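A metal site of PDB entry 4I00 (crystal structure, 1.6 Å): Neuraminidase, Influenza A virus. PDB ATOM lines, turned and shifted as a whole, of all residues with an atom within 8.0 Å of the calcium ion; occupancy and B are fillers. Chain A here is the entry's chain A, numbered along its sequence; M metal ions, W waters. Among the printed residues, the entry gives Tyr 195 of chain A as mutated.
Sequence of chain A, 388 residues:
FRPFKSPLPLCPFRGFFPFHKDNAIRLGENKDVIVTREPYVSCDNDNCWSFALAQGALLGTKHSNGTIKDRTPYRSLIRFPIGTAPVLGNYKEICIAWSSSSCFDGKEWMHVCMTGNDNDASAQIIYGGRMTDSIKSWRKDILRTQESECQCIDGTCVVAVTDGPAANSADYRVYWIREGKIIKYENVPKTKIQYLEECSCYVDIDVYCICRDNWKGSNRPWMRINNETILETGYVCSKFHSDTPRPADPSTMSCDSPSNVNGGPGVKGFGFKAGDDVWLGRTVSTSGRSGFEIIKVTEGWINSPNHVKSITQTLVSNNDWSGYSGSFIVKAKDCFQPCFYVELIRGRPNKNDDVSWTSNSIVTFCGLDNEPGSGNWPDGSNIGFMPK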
ATOM      1  N   TYR A 195       0.201 -26.753 -28.060  1.00  0.00           N
ATOM      2  CA  TYR A 195       1.016 -25.989 -27.118  1.00  0.00           C
ATOM      3  C   TYR A 195       1.607 -26.914 -26.070  1.00  0.00           C
ATOM      4  O   TYR A 195       0.925 -27.807 -25.564  1.00  0.00           O
ATOM      5  CB  TYR A 195       0.201 -24.893 -26.439  1.00  0.00           C
ATOM      6  CG  TYR A 195       1.041 -23.803 -25.814  1.00  0.00           C
ATOM      7  CD1 TYR A 195       1.188 -22.575 -26.446  1.00  0.00           C
ATOM      8  CD2 TYR A 195       1.712 -23.993 -24.602  1.00  0.00           C
ATOM      9  CE1 TYR A 195       1.952 -21.568 -25.895  1.00  0.00           C
ATOM     10  CE2 TYR A 195       2.484 -22.986 -24.044  1.00  0.00           C
ATOM     11  CZ  TYR A 195       2.595 -21.775 -24.710  1.00  0.00           C
ATOM     12  OH  TYR A 195       3.348 -20.757 -24.192  1.00  0.00           O
ATOM     13  N   CYS A 211       2.597 -32.661 -20.145  1.00  0.00           N
ATOM     14  CA  CYS A 211       2.965 -31.260 -20.034  1.00  0.00           C
ATOM     15  C   CYS A 211       1.771 -30.318 -19.855  1.00  0.00           C
ATOM     16  O   CYS A 211       0.670 -30.748 -19.488  1.00  0.00           O
ATOM     17  CB  CYS A 211       3.841 -30.835 -21.224  1.00  0.00           C
ATOM     18  SG  CYS A 211       4.990 -32.160 -21.796  1.00  0.00           S
ATOM     19  N   ARG A 212       2.022 -29.051 -20.085  1.00  0.00           N
ATOM     20  CA  ARG A 212       1.037 -27.994 -19.884  1.00  0.00           C
ATOM     21  C   ARG A 212       0.763 -27.238 -21.194  1.00  0.00           C
ATOM     22  O   ARG A 212       1.664 -26.645 -21.756  1.00  0.00           O
ATOM     23  CB  ARG A 212       1.546 -27.039 -18.805  1.00  0.00           C
ATOM     24  CG  ARG A 212       0.819 -25.725 -18.696  1.00  0.00           C
ATOM     25  CD  ARG A 212       1.494 -24.845 -17.650  1.00  0.00           C
ATOM     26  NE  ARG A 212       0.897 -23.510 -17.574  1.00  0.00           N
ATOM     27  CZ  ARG A 212       1.234 -22.591 -16.675  1.00  0.00           C
ATOM     28  NH1 ARG A 212       2.148 -22.843 -15.744  1.00  0.00           N
ATOM     29  NH2 ARG A 212       0.645 -21.397 -16.710  1.00  0.00           N
ATOM     30  N   ASP A 213      -0.479 -27.306 -21.660  1.00  0.00           N
ATOM     31  CA  ASP A 213      -0.935 -26.480 -22.780  1.00  0.00           C
ATOM     32  C   ASP A 213      -1.572 -25.258 -22.131  1.00  0.00           C
ATOM     33  O   ASP A 213      -2.537 -25.403 -21.396  1.00  0.00           O
ATOM     34  CB  ASP A 213      -1.969 -27.270 -23.585  1.00  0.00           C
ATOM     35  CG  ASP A 213      -2.630 -26.456 -24.698  1.00  0.00           C
ATOM     36  OD1 ASP A 213      -2.913 -25.261 -24.486  1.00  0.00           O
ATOM     37  OD2 ASP A 213      -2.885 -27.030 -25.789  1.00  0.00           O
ATOM     38  N   ASN A 214      -1.025 -24.072 -22.353  1.00  0.00           N
ATOM     39  CA  ASN A 214      -1.563 -22.889 -21.688  1.00  0.00           C
ATOM     40  C   ASN A 214      -2.473 -22.087 -22.606  1.00  0.00           C
ATOM     41  O   ASN A 214      -2.802 -20.944 -22.302  1.00  0.00           O
ATOM     42  CB  ASN A 214      -0.458 -21.991 -21.101  1.00  0.00           C
ATOM     43  CG  ASN A 214       0.456 -21.381 -22.159  1.00  0.00           C
ATOM     44  OD1 ASN A 214       1.641 -21.113 -21.892  1.00  0.00           O
ATOM     45  ND2 ASN A 214      -0.073 -21.130 -23.348  1.00  0.00           N
ATOM     46  N   TRP A 215      -2.867 -22.714 -23.710  1.00  0.00           N
ATOM     47  CA  TRP A 215      -3.602 -22.026 -24.767  1.00  0.00           C
ATOM     48  C   TRP A 215      -5.033 -22.560 -24.940  1.00  0.00           C
ATOM     49  O   TRP A 215      -5.969 -21.976 -24.427  1.00  0.00           O
ATOM     50  CB  TRP A 215      -2.833 -22.146 -26.094  1.00  0.00           C
ATOM     51  CG  TRP A 215      -3.349 -21.254 -27.215  1.00  0.00           C
ATOM     52  CD1 TRP A 215      -4.291 -20.267 -27.122  1.00  0.00           C
ATOM     53  CD2 TRP A 215      -2.927 -21.279 -28.584  1.00  0.00           C
ATOM     54  NE1 TRP A 215      -4.491 -19.677 -28.352  1.00  0.00           N
ATOM     55  CE2 TRP A 215      -3.659 -20.288 -29.269  1.00  0.00           C
ATOM     56  CE3 TRP A 215      -2.012 -22.049 -29.302  1.00  0.00           C
ATOM     57  CZ2 TRP A 215      -3.495 -20.039 -30.627  1.00  0.00           C
ATOM     58  CZ3 TRP A 215      -1.846 -21.806 -30.647  1.00  0.00           C
ATOM     59  CH2 TRP A 215      -2.591 -20.811 -31.306  1.00  0.00           C
ATOM     60  N   LYS A 216      -5.186 -23.673 -25.655  1.00  0.00           N
ATOM     61  CA  LYS A 216      -6.529 -24.180 -25.946  1.00  0.00           C
ATOM     62  C   LYS A 216      -6.871 -25.507 -25.253  1.00  0.00           C
ATOM     63  O   LYS A 216      -7.985 -26.000 -25.406  1.00  0.00           O
ATOM     64  CB  LYS A 216      -6.713 -24.361 -27.449  1.00  0.00           C
ATOM     65  CG  LYS A 216      -6.589 -23.083 -28.274  1.00  0.00           C
ATOM     66  CD  LYS A 216      -6.210 -23.428 -29.719  1.00  0.00           C
ATOM     67  CE  LYS A 216      -5.002 -24.382 -29.740  1.00  0.00           C
ATOM     68  NZ  LYS A 216      -4.471 -24.667 -31.101  1.00  0.00           N
ATOM     69  N   GLY A 217      -5.937 -26.081 -24.517  1.00  0.00           N
ATOM     70  CA  GLY A 217      -6.142 -27.417 -23.989  1.00  0.00           C
ATOM     71  C   GLY A 217      -6.301 -27.514 -22.477  1.00  0.00           C
ATOM     72  O   GLY A 217      -5.392 -27.175 -21.740  1.00  0.00           O
ATOM     73  N   SER A 218      -7.462 -27.982 -22.033  1.00  0.00           N
ATOM     74  CA  SER A 218      -7.649 -28.302 -20.618  1.00  0.00           C
ATOM     75  C   SER A 218      -7.183 -29.715 -20.360  1.00  0.00           C
ATOM     76  O   SER A 218      -6.956 -30.116 -19.212  1.00  0.00           O
ATOM     77  CB  SER A 218      -9.126 -28.143 -20.214  1.00  0.00           C
ATOM     78  OG  SER A 218      -9.960 -28.980 -20.991  1.00  0.00           O
ATOM     79  N   ASN A 219      -7.048 -30.501 -21.429  1.00  0.00           N
ATOM     80  CA  ASN A 219      -6.368 -31.789 -21.379  1.00  0.00           C
ATOM     81  C   ASN A 219      -4.850 -31.558 -21.527  1.00  0.00           C
ATOM     82  O   ASN A 219      -4.431 -30.532 -22.076  1.00  0.00           O
ATOM     83  CB  ASN A 219      -6.879 -32.738 -22.471  1.00  0.00           C
ATOM     84  CG  ASN A 219      -6.989 -32.075 -23.853  1.00  0.00           C
ATOM     85  OD1 ASN A 219      -6.988 -30.844 -23.986  1.00  0.00           O
ATOM     86  ND2 ASN A 219      -7.109 -32.904 -24.891  1.00  0.00           N
ATOM     87  N   ARG A 220      -4.049 -32.489 -21.043  1.00  0.00           N
ATOM     88  CA  ARG A 220      -2.599 -32.316 -21.090  1.00  0.00           C
ATOM     89  C   ARG A 220      -1.948 -32.947 -22.319  1.00  0.00           C
ATOM     90  O   ARG A 220      -2.213 -34.111 -22.635  1.00  0.00           O
ATOM     91  CB  ARG A 220      -1.942 -32.861 -19.809  1.00  0.00           C
ATOM     92  CG  ARG A 220      -2.248 -32.030 -18.586  1.00  0.00           C
ATOM     93  CD  ARG A 220      -1.312 -32.371 -17.416  1.00  0.00           C
ATOM     94  NE  ARG A 220      -1.645 -31.586 -16.233  1.00  0.00           N
ATOM     95  CZ  ARG A 220      -1.354 -30.300 -16.092  1.00  0.00           C
ATOM     96  NH1 ARG A 220      -0.703 -29.662 -17.045  1.00  0.00           N
ATOM     97  NH2 ARG A 220      -1.702 -29.651 -14.984  1.00  0.00           N
ATOM     98  N   PRO A 221      -1.054 -32.187 -22.985  1.00  0.00           N
ATOM     99  CA  PRO A 221      -0.262 -32.698 -24.109  1.00  0.00           C
ATOM    100  C   PRO A 221       0.787 -33.672 -23.601  1.00  0.00           C
ATOM    101  O   PRO A 221       1.224 -33.541 -22.461  1.00  0.00           O
ATOM    102  CB  PRO A 221       0.415 -31.447 -24.664  1.00  0.00           C
ATOM    103  CG  PRO A 221       0.473 -30.482 -23.517  1.00  0.00           C
ATOM    104  CD  PRO A 221      -0.766 -30.763 -22.696  1.00  0.00           C
ATOM    105  N   TYR A 235      -2.591 -35.756 -26.883  1.00  0.00           N
ATOM    106  CA  TYR A 235      -3.135 -35.248 -25.639  1.00  0.00           C
ATOM    107  C   TYR A 235      -3.674 -36.452 -24.871  1.00  0.00           C
ATOM    108  O   TYR A 235      -4.044 -37.473 -25.476  1.00  0.00           O
ATOM    109  CB  TYR A 235      -4.232 -34.223 -25.890  1.00  0.00           C
ATOM    110  CG  TYR A 235      -3.736 -32.839 -26.274  1.00  0.00           C
ATOM    111  CD1 TYR A 235      -3.411 -32.536 -27.598  1.00  0.00           C
ATOM    112  CD2 TYR A 235      -3.615 -31.848 -25.320  1.00  0.00           C
ATOM    113  CE1 TYR A 235      -2.962 -31.267 -27.941  1.00  0.00           C
ATOM    114  CE2 TYR A 235      -3.164 -30.585 -25.650  1.00  0.00           C
ATOM    115  CZ  TYR A 235      -2.838 -30.301 -26.960  1.00  0.00           C
ATOM    116  OH  TYR A 235      -2.391 -29.030 -27.285  1.00  0.00           O
ATOM    117  N   SER A 242      -7.116 -32.836 -16.631  1.00  0.00           N
ATOM    118  CA  SER A 242      -6.286 -32.664 -15.434  1.00  0.00           C
ATOM    119  C   SER A 242      -5.452 -31.379 -15.370  1.00  0.00           C
ATOM    120  O   SER A 242      -4.611 -31.242 -14.480  1.00  0.00           O
ATOM    121  CB  SER A 242      -5.402 -33.900 -15.225  1.00  0.00           C
ATOM    122  OG  SER A 242      -4.492 -34.046 -16.295  1.00  0.00           O
ATOM    123  N   ASP A 243      -5.680 -30.447 -16.286  1.00  0.00           N
ATOM    124  CA  ASP A 243      -5.090 -29.130 -16.150  1.00  0.00           C
ATOM    125  C   ASP A 243      -5.977 -28.270 -15.254  1.00  0.00           C
ATOM    126  O   ASP A 243      -7.039 -28.723 -14.824  1.00  0.00           O
ATOM    127  CB  ASP A 243      -4.858 -28.458 -17.522  1.00  0.00           C
ATOM    128  CG  ASP A 243      -3.671 -27.493 -17.519  1.00  0.00           C
ATOM    129  OD1 ASP A 243      -3.157 -27.155 -16.414  1.00  0.00           O
ATOM    130  OD2 ASP A 243      -3.235 -27.068 -18.608  1.00  0.00           O
ATOM    131  N   THR A 244      -5.531 -27.060 -14.966  1.00  0.00           N
ATOM    132  CA  THR A 244      -6.289 -26.103 -14.177  1.00  0.00           C
ATOM    133  C   THR A 244      -6.137 -24.711 -14.798  1.00  0.00           C
ATOM    134  O   THR A 244      -5.037 -24.172 -14.889  1.00  0.00           O
ATOM    135  CB  THR A 244      -5.779 -26.052 -12.708  1.00  0.00           C
ATOM    136  OG1 THR A 244      -5.800 -27.362 -12.139  1.00  0.00           O
ATOM    137  CG2 THR A 244      -6.629 -25.115 -11.869  1.00  0.00           C
ATOM    138  N   PRO A 245      -7.252 -24.089 -15.229  1.00  0.00           N
ATOM    139  CA  PRO A 245      -8.652 -24.513 -15.114  1.00  0.00           C
ATOM    140  C   PRO A 245      -9.013 -25.663 -16.044  1.00  0.00           C
ATOM    141  O   PRO A 245      -8.210 -26.073 -16.889  1.00  0.00           O
ATOM    142  CB  PRO A 245      -9.429 -23.251 -15.491  1.00  0.00           C
ATOM    143  CG  PRO A 245      -8.509 -22.538 -16.448  1.00  0.00           C
ATOM    144  CD  PRO A 245      -7.141 -22.768 -15.860  1.00  0.00           C
ATOM    145  N   ARG A 246     -10.221 -26.192 -15.902  1.00  0.00           N
ATOM    146  CA  ARG A 246     -10.672 -27.281 -16.760  1.00  0.00           C
ATOM    147  C   ARG A 246     -12.172 -27.422 -16.567  1.00  0.00           C
ATOM    148  O   ARG A 246     -12.721 -26.895 -15.603  1.00  0.00           O
ATOM    149  CB  ARG A 246      -9.998 -28.585 -16.349  1.00  0.00           C
ATOM    150  CG  ARG A 246     -10.245 -28.955 -14.886  1.00  0.00           C
ATOM    151  CD  ARG A 246      -9.792 -30.354 -14.572  1.00  0.00           C
ATOM    152  NE  ARG A 246     -10.143 -30.737 -13.202  1.00  0.00           N
ATOM    153  CZ  ARG A 246      -9.409 -30.440 -12.130  1.00  0.00           C
ATOM    154  NH1 ARG A 246      -9.830 -30.825 -10.931  1.00  0.00           N
ATOM    155  NH2 ARG A 246      -8.260 -29.779 -12.251  1.00  0.00           N
ATOM    156  N   SER A 259      -8.585 -29.701 -25.983  1.00  0.00           N
ATOM    157  CA  SER A 259     -10.025 -29.787 -25.726  1.00  0.00           C
ATOM    158  C   SER A 259     -10.764 -28.593 -26.319  1.00  0.00           C
ATOM    159  O   SER A 259     -11.986 -28.647 -26.524  1.00  0.00           O
ATOM    160  CB  SER A 259     -10.284 -29.861 -24.229  1.00  0.00           C
ATOM    161  OG  SER A 259     -10.008 -28.609 -23.632  1.00  0.00           O
ATOM    162  N   VAL A 261     -11.357 -25.907 -24.773  1.00  0.00           N
ATOM    163  CA  VAL A 261     -12.135 -25.261 -23.715  1.00  0.00           C
ATOM    164  C   VAL A 261     -11.290 -25.146 -22.444  1.00  0.00           C
ATOM    165  O   VAL A 261     -10.470 -26.014 -22.153  1.00  0.00           O
ATOM    166  CB  VAL A 261     -13.413 -26.047 -23.413  1.00  0.00           C
ATOM    167  CG1 VAL A 261     -13.068 -27.459 -22.934  1.00  0.00           C
ATOM    168  CG2 VAL A 261     -14.271 -25.305 -22.410  1.00  0.00           C
ATOM    169  N   ASN A 262     -11.506 -24.063 -21.683  1.00  0.00           N
ATOM    170  CA  ASN A 262     -10.743 -23.773 -20.470  1.00  0.00           C
ATOM    171  C   ASN A 262      -9.238 -23.990 -20.615  1.00  0.00           C
ATOM    172  O   ASN A 262      -8.594 -24.594 -19.743  1.00  0.00           O
ATOM    173  CB  ASN A 262     -11.275 -24.598 -19.297  1.00  0.00           C
ATOM    174  CG  ASN A 262     -12.739 -24.334 -19.027  1.00  0.00           C
ATOM    175  OD1 ASN A 262     -13.126 -23.269 -18.547  1.00  0.00           O
ATOM    176  ND2 ASN A 262     -13.581 -25.319 -19.346  1.00  0.00           N
ATOM    177  N   GLY A 263      -8.673 -23.477 -21.698  1.00  0.00           N
ATOM    178  CA  GLY A 263      -7.291 -23.739 -22.042  1.00  0.00           C
ATOM    179  C   GLY A 263      -6.223 -22.990 -21.267  1.00  0.00           C
ATOM    180  O   GLY A 263      -5.093 -23.438 -21.190  1.00  0.00           O
ATOM    181  N   GLY A 264      -6.556 -21.832 -20.706  1.00  0.00           N
ATOM    182  CA  GLY A 264      -5.546 -21.010 -20.062  1.00  0.00           C
ATOM    183  C   GLY A 264      -5.909 -20.583 -18.653  1.00  0.00           C
ATOM    184  O   GLY A 264      -7.092 -20.535 -18.308  1.00  0.00           O
ATOM    185  N   PRO A 265      -4.899 -20.254 -17.832  1.00  0.00           N
ATOM    186  CA  PRO A 265      -3.472 -20.261 -18.169  1.00  0.00           C
ATOM    187  C   PRO A 265      -2.794 -21.603 -17.900  1.00  0.00           C
ATOM    188  O   PRO A 265      -1.651 -21.814 -18.320  1.00  0.00           O
ATOM    189  CB  PRO A 265      -2.912 -19.214 -17.204  1.00  0.00           C
ATOM    190  CG  PRO A 265      -3.744 -19.402 -15.975  1.00  0.00           C
ATOM    191  CD  PRO A 265      -5.129 -19.765 -16.461  1.00  0.00           C
ATOM    192  N   GLY A 266      -3.478 -22.502 -17.193  1.00  0.00           N
ATOM    193  CA  GLY A 266      -2.934 -23.824 -16.920  1.00  0.00           C
ATOM    194  C   GLY A 266      -1.992 -23.841 -15.723  1.00  0.00           C
ATOM    195  O   GLY A 266      -1.709 -22.810 -15.117  1.00  0.00           O
ATOM    196  N   VAL A 267      -1.533 -25.038 -15.373  1.00  0.00           N
ATOM    197  CA  VAL A 267      -0.588 -25.217 -14.280  1.00  0.00           C
ATOM    198  C   VAL A 267       0.290 -26.420 -14.618  1.00  0.00           C
ATOM    199  O   VAL A 267      -0.159 -27.330 -15.279  1.00  0.00           O
ATOM    200  CB  VAL A 267      -1.315 -25.473 -12.925  1.00  0.00           C
ATOM    201  CG1 VAL A 267      -2.059 -26.794 -12.963  1.00  0.00           C
ATOM    202  CG2 VAL A 267      -0.344 -25.450 -11.745  1.00  0.00           C
HETATM  203 CA    CA M   1      -4.456 -25.634 -20.096  1.00  0.00          CA
HETATM  204  O   HOH W   1      -6.376 -24.952 -18.409  1.00  0.00           O
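The backbone carbonyl oxygen (O) of Thr 244 lies close to the backbone NH (N) of Gly 266, at 3.2 Å.
N of Lys 216 lies within hydrogen-bond range of OD1 of Asp 213 (3.0 Å).
O of Gly 266 is in hydrogen-bond range of NH2 of Arg 212, at 3.2 Å.
O of Asp 243 sits at hydrogen-bond distance from NH2 of Arg 246.
N of Asp 243 lies close to O of Ser 218.
The side-chain carboxylate of Asp 213 lies within hydrogen-bond range of the backbone NH of Trp 215 (2.7 Å).
The side-chain carboxylate (OD2) of Asp 213 lies within hydrogen-bond range of the side-chain hydroxyl (OH) of Tyr 235.
O of Gly 263 lies close to N of Trp 215, at 3.4 Å.
Residues that only touch the calcium ion: Gly 266 (3.96 Å).
The nearest printed residue that does not touch the calcium ion is Ser 218 (4.2 Å).
The calcium ion is bound by the backbone carbonyl oxygen of Asp 213 (2.3 Å), the side-chain carboxylate of Asp 243 (2.4 Å), the backbone carbonyl oxygen of Gly 217 (2.4 Å), the backbone carbonyl oxygen of Gly 263 (2.5 Å) and water W1 (2.6 Å).
The calcium ion has five donor atoms within binding distance.
Water W1 lies within hydrogen-bond range of O of Asn 262 and O of Pro 245.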
